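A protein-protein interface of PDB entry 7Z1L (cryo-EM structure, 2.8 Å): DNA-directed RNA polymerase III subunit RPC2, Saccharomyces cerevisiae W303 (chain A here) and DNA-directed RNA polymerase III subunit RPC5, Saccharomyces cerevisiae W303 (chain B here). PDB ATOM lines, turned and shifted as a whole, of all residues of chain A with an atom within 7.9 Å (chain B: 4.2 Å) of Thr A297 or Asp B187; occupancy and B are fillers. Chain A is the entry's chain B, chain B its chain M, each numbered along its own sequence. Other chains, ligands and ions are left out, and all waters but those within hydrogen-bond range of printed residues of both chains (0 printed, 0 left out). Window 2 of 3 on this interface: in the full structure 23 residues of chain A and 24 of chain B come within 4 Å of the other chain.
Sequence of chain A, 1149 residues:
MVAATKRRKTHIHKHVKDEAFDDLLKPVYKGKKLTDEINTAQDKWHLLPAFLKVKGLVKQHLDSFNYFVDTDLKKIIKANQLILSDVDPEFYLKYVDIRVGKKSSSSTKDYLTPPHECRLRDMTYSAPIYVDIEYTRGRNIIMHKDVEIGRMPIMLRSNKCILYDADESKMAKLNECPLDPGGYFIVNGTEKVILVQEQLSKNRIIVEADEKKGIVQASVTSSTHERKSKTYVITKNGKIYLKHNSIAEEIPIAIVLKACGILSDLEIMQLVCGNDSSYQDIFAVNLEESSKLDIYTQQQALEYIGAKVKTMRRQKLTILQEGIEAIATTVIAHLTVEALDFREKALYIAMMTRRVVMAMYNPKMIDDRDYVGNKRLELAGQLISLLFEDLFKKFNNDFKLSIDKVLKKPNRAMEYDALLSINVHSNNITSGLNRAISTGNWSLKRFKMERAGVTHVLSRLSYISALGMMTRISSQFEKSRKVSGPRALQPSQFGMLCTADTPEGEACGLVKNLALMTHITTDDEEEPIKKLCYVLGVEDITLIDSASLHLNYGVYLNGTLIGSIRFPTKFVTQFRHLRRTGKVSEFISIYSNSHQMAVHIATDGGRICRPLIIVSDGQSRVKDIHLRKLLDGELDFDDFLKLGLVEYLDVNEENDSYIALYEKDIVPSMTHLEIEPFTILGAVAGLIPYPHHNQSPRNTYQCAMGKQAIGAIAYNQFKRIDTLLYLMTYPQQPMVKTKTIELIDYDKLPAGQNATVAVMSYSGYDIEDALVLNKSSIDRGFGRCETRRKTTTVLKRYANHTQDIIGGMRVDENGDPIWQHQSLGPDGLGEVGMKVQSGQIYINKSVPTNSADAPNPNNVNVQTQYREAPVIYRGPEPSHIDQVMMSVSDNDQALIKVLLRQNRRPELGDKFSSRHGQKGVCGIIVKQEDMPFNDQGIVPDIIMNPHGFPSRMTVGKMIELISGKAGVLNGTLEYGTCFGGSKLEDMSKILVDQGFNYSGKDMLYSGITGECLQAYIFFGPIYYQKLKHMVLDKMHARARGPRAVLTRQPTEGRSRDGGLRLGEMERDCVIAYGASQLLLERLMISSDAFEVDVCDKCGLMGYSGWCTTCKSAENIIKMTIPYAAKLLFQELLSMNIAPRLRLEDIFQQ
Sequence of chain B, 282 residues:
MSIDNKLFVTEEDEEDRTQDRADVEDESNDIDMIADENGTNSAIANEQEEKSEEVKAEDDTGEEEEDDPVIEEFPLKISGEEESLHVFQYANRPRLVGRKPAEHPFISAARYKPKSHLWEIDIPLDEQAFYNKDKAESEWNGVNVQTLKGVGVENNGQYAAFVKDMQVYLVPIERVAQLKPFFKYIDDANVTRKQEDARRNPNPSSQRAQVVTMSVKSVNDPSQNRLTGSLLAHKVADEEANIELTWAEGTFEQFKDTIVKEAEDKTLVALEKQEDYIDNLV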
ATOM      1  N   ILE A 255     -15.348  -6.090 -31.037  1.00  0.00           N
ATOM      2  CA  ILE A 255     -14.823  -5.364 -29.882  1.00  0.00           C
ATOM      3  C   ILE A 255     -14.030  -4.142 -30.330  1.00  0.00           C
ATOM      4  O   ILE A 255     -14.167  -3.050 -29.764  1.00  0.00           O
ATOM      5  CB  ILE A 255     -13.975  -6.299 -29.003  1.00  0.00           C
ATOM      6  CG1 ILE A 255     -14.773  -7.546 -28.618  1.00  0.00           C
ATOM      7  CG2 ILE A 255     -13.507  -5.576 -27.757  1.00  0.00           C
ATOM      8  CD1 ILE A 255     -16.113  -7.248 -27.983  1.00  0.00           C
ATOM      9  N   LYS A 258     -16.323  -1.549 -31.569  1.00  0.00           N
ATOM     10  CA  LYS A 258     -16.989  -0.875 -30.459  1.00  0.00           C
ATOM     11  C   LYS A 258     -16.042   0.054 -29.715  1.00  0.00           C
ATOM     12  O   LYS A 258     -16.496   0.993 -29.052  1.00  0.00           O
ATOM     13  CB  LYS A 258     -17.583  -1.901 -29.497  1.00  0.00           C
ATOM     14  CG  LYS A 258     -18.959  -2.396 -29.893  1.00  0.00           C
ATOM     15  CD  LYS A 258     -19.418  -3.514 -28.979  1.00  0.00           C
ATOM     16  CE  LYS A 258     -20.363  -4.454 -29.699  1.00  0.00           C
ATOM     17  NZ  LYS A 258     -21.582  -3.750 -30.177  1.00  0.00           N
ATOM     18  N   ALA A 259     -14.733  -0.198 -29.796  1.00  0.00           N
ATOM     19  CA  ALA A 259     -13.766   0.711 -29.188  1.00  0.00           C
ATOM     20  C   ALA A 259     -13.797   2.078 -29.851  1.00  0.00           C
ATOM     21  O   ALA A 259     -13.513   3.091 -29.202  1.00  0.00           O
ATOM     22  CB  ALA A 259     -12.362   0.117 -29.263  1.00  0.00           C
ATOM     23  N   CYS A 260     -14.136   2.128 -31.134  1.00  0.00           N
ATOM     24  CA  CYS A 260     -14.325   3.385 -31.840  1.00  0.00           C
ATOM     25  C   CYS A 260     -15.722   3.925 -31.534  1.00  0.00           C
ATOM     26  O   CYS A 260     -16.399   3.481 -30.603  1.00  0.00           O
ATOM     27  CB  CYS A 260     -14.087   3.189 -33.333  1.00  0.00           C
ATOM     28  SG  CYS A 260     -12.583   2.271 -33.733  1.00  0.00           S
ATOM     29  N   ILE A 262     -18.560   3.596 -32.960  1.00  0.00           N
ATOM     30  CA  ILE A 262     -19.716   2.750 -33.243  1.00  0.00           C
ATOM     31  C   ILE A 262     -20.066   1.959 -31.989  1.00  0.00           C
ATOM     32  O   ILE A 262     -19.203   1.310 -31.392  1.00  0.00           O
ATOM     33  CB  ILE A 262     -19.440   1.810 -34.423  1.00  0.00           C
ATOM     34  CG1 ILE A 262     -18.974   2.602 -35.640  1.00  0.00           C
ATOM     35  CG2 ILE A 262     -20.684   1.024 -34.770  1.00  0.00           C
ATOM     36  CD1 ILE A 262     -18.507   1.728 -36.772  1.00  0.00           C
ATOM     37  N   LEU A 263     -21.335   2.014 -31.587  1.00  0.00           N
ATOM     38  CA  LEU A 263     -21.802   1.300 -30.408  1.00  0.00           C
ATOM     39  C   LEU A 263     -22.995   0.395 -30.681  1.00  0.00           C
ATOM     40  O   LEU A 263     -23.531  -0.197 -29.739  1.00  0.00           O
ATOM     41  CB  LEU A 263     -22.155   2.291 -29.291  1.00  0.00           C
ATOM     42  CG  LEU A 263     -20.956   3.020 -28.687  1.00  0.00           C
ATOM     43  CD1 LEU A 263     -21.402   4.087 -27.702  1.00  0.00           C
ATOM     44  CD2 LEU A 263     -20.025   2.026 -28.022  1.00  0.00           C
ATOM     45  N   ASP A 294     -19.240 -10.174 -22.938  1.00  0.00           N
ATOM     46  CA  ASP A 294     -20.058  -9.144 -22.282  1.00  0.00           C
ATOM     47  C   ASP A 294     -19.460  -7.739 -22.355  1.00  0.00           C
ATOM     48  O   ASP A 294     -19.347  -7.042 -21.341  1.00  0.00           O
ATOM     49  CB  ASP A 294     -20.436  -9.525 -20.829  1.00  0.00           C
ATOM     50  CG  ASP A 294     -19.254  -9.665 -19.862  1.00  0.00           C
ATOM     51  OD1 ASP A 294     -18.081  -9.519 -20.227  1.00  0.00           O
ATOM     52  OD2 ASP A 294     -19.530  -9.935 -18.675  1.00  0.00           O
ATOM     53  N   ILE A 295     -19.091  -7.316 -23.561  1.00  0.00           N
ATOM     54  CA  ILE A 295     -18.642  -5.956 -23.840  1.00  0.00           C
ATOM     55  C   ILE A 295     -19.728  -5.271 -24.653  1.00  0.00           C
ATOM     56  O   ILE A 295     -20.086  -5.741 -25.740  1.00  0.00           O
ATOM     57  CB  ILE A 295     -17.305  -5.941 -24.593  1.00  0.00           C
ATOM     58  CG1 ILE A 295     -16.204  -6.560 -23.736  1.00  0.00           C
ATOM     59  CG2 ILE A 295     -16.947  -4.528 -25.010  1.00  0.00           C
ATOM     60  CD1 ILE A 295     -14.929  -6.821 -24.487  1.00  0.00           C
ATOM     61  N   TYR A 296     -20.253  -4.162 -24.135  1.00  0.00           N
ATOM     62  CA  TYR A 296     -21.364  -3.485 -24.790  1.00  0.00           C
ATOM     63  C   TYR A 296     -21.201  -1.978 -24.911  1.00  0.00           C
ATOM     64  O   TYR A 296     -21.915  -1.369 -25.716  1.00  0.00           O
ATOM     65  CB  TYR A 296     -22.675  -3.785 -24.052  1.00  0.00           C
ATOM     66  CG  TYR A 296     -23.101  -5.228 -24.183  1.00  0.00           C
ATOM     67  CD1 TYR A 296     -22.780  -6.153 -23.200  1.00  0.00           C
ATOM     68  CD2 TYR A 296     -23.777  -5.676 -25.308  1.00  0.00           C
ATOM     69  CE1 TYR A 296     -23.156  -7.475 -23.316  1.00  0.00           C
ATOM     70  CE2 TYR A 296     -24.158  -6.995 -25.433  1.00  0.00           C
ATOM     71  CZ  TYR A 296     -23.841  -7.891 -24.435  1.00  0.00           C
ATOM     72  OH  TYR A 296     -24.214  -9.210 -24.556  1.00  0.00           O
ATOM     73  N   THR A 297     -20.303  -1.356 -24.154  1.00  0.00           N
ATOM     74  CA  THR A 297     -20.055   0.074 -24.251  1.00  0.00           C
ATOM     75  C   THR A 297     -18.631   0.326 -24.728  1.00  0.00           C
ATOM     76  O   THR A 297     -17.797  -0.581 -24.776  1.00  0.00           O
ATOM     77  CB  THR A 297     -20.294   0.771 -22.907  1.00  0.00           C
ATOM     78  OG1 THR A 297     -20.391   2.185 -23.112  1.00  0.00           O
ATOM     79  CG2 THR A 297     -19.159   0.483 -21.943  1.00  0.00           C
ATOM     80  N   GLN A 298     -18.370   1.583 -25.099  1.00  0.00           N
ATOM     81  CA  GLN A 298     -17.057   1.952 -25.620  1.00  0.00           C
ATOM     82  C   GLN A 298     -15.975   1.808 -24.557  1.00  0.00           C
ATOM     83  O   GLN A 298     -14.857   1.367 -24.852  1.00  0.00           O
ATOM     84  CB  GLN A 298     -17.093   3.382 -26.160  1.00  0.00           C
ATOM     85  CG  GLN A 298     -15.790   3.848 -26.781  1.00  0.00           C
ATOM     86  CD  GLN A 298     -15.939   5.152 -27.534  1.00  0.00           C
ATOM     87  OE1 GLN A 298     -16.929   5.863 -27.376  1.00  0.00           O
ATOM     88  NE2 GLN A 298     -14.952   5.472 -28.362  1.00  0.00           N
ATOM     89  N   GLN A 299     -16.292   2.178 -23.314  1.00  0.00           N
ATOM     90  CA  GLN A 299     -15.312   2.091 -22.237  1.00  0.00           C
ATOM     91  C   GLN A 299     -14.922   0.645 -21.957  1.00  0.00           C
ATOM     92  O   GLN A 299     -13.756   0.358 -21.668  1.00  0.00           O
ATOM     93  CB  GLN A 299     -15.858   2.757 -20.976  1.00  0.00           C
ATOM     94  CG  GLN A 299     -14.809   3.018 -19.911  1.00  0.00           C
ATOM     95  CD  GLN A 299     -15.260   4.043 -18.890  1.00  0.00           C
ATOM     96  OE1 GLN A 299     -16.080   4.912 -19.186  1.00  0.00           O
ATOM     97  NE2 GLN A 299     -14.726   3.946 -17.679  1.00  0.00           N
ATOM     98  N   GLN A 300     -15.882  -0.280 -22.043  1.00  0.00           N
ATOM     99  CA  GLN A 300     -15.579  -1.692 -21.827  1.00  0.00           C
ATOM    100  C   GLN A 300     -14.631  -2.228 -22.894  1.00  0.00           C
ATOM    101  O   GLN A 300     -13.679  -2.955 -22.583  1.00  0.00           O
ATOM    102  CB  GLN A 300     -16.871  -2.506 -21.808  1.00  0.00           C
ATOM    103  CG  GLN A 300     -17.568  -2.537 -20.464  1.00  0.00           C
ATOM    104  CD  GLN A 300     -18.879  -3.292 -20.513  1.00  0.00           C
ATOM    105  OE1 GLN A 300     -19.625  -3.197 -21.485  1.00  0.00           O
ATOM    106  NE2 GLN A 300     -19.167  -4.049 -19.461  1.00  0.00           N
ATOM    107  N   ALA A 301     -14.872  -1.872 -24.158  1.00  0.00           N
ATOM    108  CA  ALA A 301     -13.988  -2.312 -25.233  1.00  0.00           C
ATOM    109  C   ALA A 301     -12.608  -1.685 -25.101  1.00  0.00           C
ATOM    110  O   ALA A 301     -11.594  -2.330 -25.392  1.00  0.00           O
ATOM    111  CB  ALA A 301     -14.604  -1.976 -26.589  1.00  0.00           C
ATOM    112  N   LEU A 302     -12.550  -0.425 -24.659  1.00  0.00           N
ATOM    113  CA  LEU A 302     -11.259   0.216 -24.439  1.00  0.00           C
ATOM    114  C   LEU A 302     -10.490  -0.453 -23.303  1.00  0.00           C
ATOM    115  O   LEU A 302      -9.274  -0.643 -23.405  1.00  0.00           O
ATOM    116  CB  LEU A 302     -11.457   1.705 -24.169  1.00  0.00           C
ATOM    117  CG  LEU A 302     -11.761   2.531 -25.420  1.00  0.00           C
ATOM    118  CD1 LEU A 302     -12.308   3.898 -25.050  1.00  0.00           C
ATOM    119  CD2 LEU A 302     -10.521   2.664 -26.287  1.00  0.00           C
ATOM    120  N   GLU A 303     -11.183  -0.821 -22.218  1.00  0.00           N
ATOM    121  CA  GLU A 303     -10.556  -1.603 -21.153  1.00  0.00           C
ATOM    122  C   GLU A 303     -10.025  -2.928 -21.679  1.00  0.00           C
ATOM    123  O   GLU A 303      -8.892  -3.323 -21.376  1.00  0.00           O
ATOM    124  CB  GLU A 303     -11.554  -1.870 -20.021  1.00  0.00           C
ATOM    125  CG  GLU A 303     -12.023  -0.669 -19.228  1.00  0.00           C
ATOM    126  CD  GLU A 303     -10.916  -0.040 -18.414  1.00  0.00           C
ATOM    127  OE1 GLU A 303     -10.009  -0.774 -17.972  1.00  0.00           O
ATOM    128  OE2 GLU A 303     -10.971   1.184 -18.186  1.00  0.00           O
ATOM    129  N   LEU A 320      -7.568   2.389 -19.162  1.00  0.00           N
ATOM    130  CA  LEU A 320      -8.486   3.017 -20.110  1.00  0.00           C
ATOM    131  C   LEU A 320      -7.741   3.960 -21.043  1.00  0.00           C
ATOM    132  O   LEU A 320      -7.964   3.960 -22.259  1.00  0.00           O
ATOM    133  CB  LEU A 320      -9.580   3.776 -19.358  1.00  0.00           C
ATOM    134  CG  LEU A 320     -10.478   4.703 -20.180  1.00  0.00           C
ATOM    135  CD1 LEU A 320     -11.246   3.924 -21.231  1.00  0.00           C
ATOM    136  CD2 LEU A 320     -11.428   5.473 -19.277  1.00  0.00           C
ATOM    137  N   PHE B 183     -24.607   3.745 -22.568  1.00  0.00           N
ATOM    138  CA  PHE B 183     -24.939   2.774 -21.532  1.00  0.00           C
ATOM    139  C   PHE B 183     -24.215   3.111 -20.237  1.00  0.00           C
ATOM    140  O   PHE B 183     -23.508   2.284 -19.659  1.00  0.00           O
ATOM    141  CB  PHE B 183     -24.616   1.361 -22.002  1.00  0.00           C
ATOM    142  CG  PHE B 183     -25.380   0.948 -23.225  1.00  0.00           C
ATOM    143  CD1 PHE B 183     -26.747   1.142 -23.299  1.00  0.00           C
ATOM    144  CD2 PHE B 183     -24.728   0.377 -24.304  1.00  0.00           C
ATOM    145  CE1 PHE B 183     -27.454   0.767 -24.423  1.00  0.00           C
ATOM    146  CE2 PHE B 183     -25.429   0.000 -25.432  1.00  0.00           C
ATOM    147  CZ  PHE B 183     -26.794   0.196 -25.492  1.00  0.00           C
ATOM    148  N   LYS B 184     -24.363   4.364 -19.792  1.00  0.00           N
ATOM    149  CA  LYS B 184     -23.661   4.844 -18.603  1.00  0.00           C
ATOM    150  C   LYS B 184     -23.985   4.030 -17.357  1.00  0.00           C
ATOM    151  O   LYS B 184     -23.146   3.924 -16.456  1.00  0.00           O
ATOM    152  CB  LYS B 184     -23.998   6.315 -18.355  1.00  0.00           C
ATOM    153  CG  LYS B 184     -25.486   6.624 -18.399  1.00  0.00           C
ATOM    154  CD  LYS B 184     -25.824   7.857 -17.578  1.00  0.00           C
ATOM    155  CE  LYS B 184     -24.976   9.050 -17.984  1.00  0.00           C
ATOM    156  NZ  LYS B 184     -25.360  10.280 -17.238  1.00  0.00           N
ATOM    157  N   TYR B 185     -25.188   3.452 -17.280  1.00  0.00           N
ATOM    158  CA  TYR B 185     -25.523   2.634 -16.119  1.00  0.00           C
ATOM    159  C   TYR B 185     -24.697   1.355 -16.077  1.00  0.00           C
ATOM    160  O   TYR B 185     -24.354   0.881 -14.989  1.00  0.00           O
ATOM    161  CB  TYR B 185     -27.018   2.312 -16.096  1.00  0.00           C
ATOM    162  CG  TYR B 185     -27.609   1.859 -17.412  1.00  0.00           C
ATOM    163  CD1 TYR B 185     -27.544   0.531 -17.805  1.00  0.00           C
ATOM    164  CD2 TYR B 185     -28.256   2.758 -18.250  1.00  0.00           C
ATOM    165  CE1 TYR B 185     -28.092   0.112 -19.001  1.00  0.00           C
ATOM    166  CE2 TYR B 185     -28.807   2.349 -19.446  1.00  0.00           C
ATOM    167  CZ  TYR B 185     -28.722   1.025 -19.818  1.00  0.00           C
ATOM    168  OH  TYR B 185     -29.269   0.612 -21.010  1.00  0.00           O
ATOM    169  N   ILE B 186     -24.353   0.798 -17.241  1.00  0.00           N
ATOM    170  CA  ILE B 186     -23.494  -0.384 -17.281  1.00  0.00           C
ATOM    171  C   ILE B 186     -22.112  -0.052 -16.731  1.00  0.00           C
ATOM    172  O   ILE B 186     -21.545  -0.805 -15.930  1.00  0.00           O
ATOM    173  CB  ILE B 186     -23.415  -0.941 -18.715  1.00  0.00           C
ATOM    174  CG1 ILE B 186     -24.788  -1.440 -19.167  1.00  0.00           C
ATOM    175  CG2 ILE B 186     -22.394  -2.062 -18.801  1.00  0.00           C
ATOM    176  CD1 ILE B 186     -24.787  -2.081 -20.536  1.00  0.00           C
ATOM    177  N   ASP B 187     -21.558   1.092 -17.140  1.00  0.00           N
ATOM    178  CA  ASP B 187     -20.248   1.505 -16.645  1.00  0.00           C
ATOM    179  C   ASP B 187     -20.288   1.826 -15.154  1.00  0.00           C
ATOM    180  O   ASP B 187     -19.341   1.513 -14.423  1.00  0.00           O
ATOM    181  CB  ASP B 187     -19.741   2.707 -17.440  1.00  0.00           C
ATOM    182  CG  ASP B 187     -18.877   2.304 -18.617  1.00  0.00           C
ATOM    183  OD1 ASP B 187     -18.122   1.317 -18.491  1.00  0.00           O
ATOM    184  OD2 ASP B 187     -18.952   2.975 -19.669  1.00  0.00           O
ATOM    185  N   ASP B 188     -21.370   2.457 -14.690  1.00  0.00           N
ATOM    186  CA  ASP B 188     -21.509   2.739 -13.264  1.00  0.00           C
ATOM    187  C   ASP B 188     -21.594   1.453 -12.451  1.00  0.00           C
ATOM    188  O   ASP B 188     -20.968   1.339 -11.391  1.00  0.00           O
ATOM    189  CB  ASP B 188     -22.737   3.613 -13.016  1.00  0.00           C
ATOM    190  CG  ASP B 188     -22.595   5.001 -13.607  1.00  0.00           C
ATOM    191  OD1 ASP B 188     -21.446   5.435 -13.837  1.00  0.00           O
ATOM    192  OD2 ASP B 188     -23.629   5.658 -13.843  1.00  0.00           O
ATOM    193  N   ALA B 189     -22.357   0.470 -12.937  1.00  0.00           N
ATOM    194  CA  ALA B 189     -22.431  -0.818 -12.257  1.00  0.00           C
ATOM    195  C   ALA B 189     -21.076  -1.512 -12.246  1.00  0.00           C
ATOM    196  O   ALA B 189     -20.681  -2.101 -11.232  1.00  0.00           O
ATOM    197  CB  ALA B 189     -23.483  -1.704 -12.922  1.00  0.00           C
ATOM    198  N   ASN B 190     -20.345  -1.441 -13.361  1.00  0.00           N
ATOM    199  CA  ASN B 190     -19.029  -2.068 -13.435  1.00  0.00           C
ATOM    200  C   ASN B 190     -18.052  -1.430 -12.454  1.00  0.00           C
ATOM    201  O   ASN B 190     -17.314  -2.132 -11.754  1.00  0.00           O
ATOM    202  CB  ASN B 190     -18.489  -1.985 -14.864  1.00  0.00           C
ATOM    203  CG  ASN B 190     -18.927  -3.157 -15.720  1.00  0.00           C
ATOM    204  OD1 ASN B 190     -19.585  -2.979 -16.744  1.00  0.00           O
ATOM    205  ND2 ASN B 190     -18.564  -4.363 -15.302  1.00  0.00           N
ATOM    206  N   VAL B 191     -18.039  -0.097 -12.379  1.00  0.00           N
ATOM    207  CA  VAL B 191     -17.086   0.568 -11.493  1.00  0.00           C
ATOM    208  C   VAL B 191     -17.485   0.379 -10.030  1.00  0.00           C
ATOM    209  O   VAL B 191     -16.621   0.264  -9.153  1.00  0.00           O
ATOM    210  CB  VAL B 191     -16.920   2.054 -11.879  1.00  0.00           C
ATOM    211  CG1 VAL B 191     -18.154   2.881 -11.549  1.00  0.00           C
ATOM    212  CG2 VAL B 191     -15.683   2.644 -11.211  1.00  0.00           C
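OD1 of Asn B190 sits close to O of Ile B186 (3.0 Å).
The side-chain amide oxygen (OE1) of Gln A300 lies within hydrogen-bond range of the backbone NH (N) of Tyr A296, at 2.9 Å.
The backbone NH (N) of Thr A297 sits at hydrogen-bond distance from the side-chain amide oxygen (OE1) of Gln A300 (3.3 Å).
The side-chain amide oxygen of Gln A299 lies close to the side-chain carboxylate of Asp B187.
The side-chain amide oxygen (OD1) of Asn B190 lies within hydrogen-bond range of the side-chain amide nitrogen (NE2) of Gln A300 (2.9 Å).
Ile A255 touches none of the printed residues of chain B.
Lys A258 touches none of the printed residues of chain B.
Of the printed residues of chain B, Tyr A296 touches Phe B183.
Thr A297 touches one residue of chain B.
Printed residues of chain B within 4 Å of Gln A299: Asp B187 (3.4 Å).
Of the printed residues of chain A, Ile B186 touches Gln A300.
Asp B187 touches just these residues of chain A: Thr A297 and Gln A299.
Printed residues of chain B that touch a printed residue of chain A: Phe B183, Ile B186, Asp B187 and Asn B190.
Hydrophobic or aromatic side chains of chain B that line the printed part of chain A: Phe B183 and Ile B186.
Among the printed residues, 5 pairs touch across the chains.
Among the printed residues, no Asp or Glu carboxylate lies within 4 Å of a Lys or Arg side-chain nitrogen of the other chain.
Among the printed residues, pairs that only touch across the chains: Thr A297 with Asp B187, Tyr A296 with Phe B183 and Gln A300 with Ile B186.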
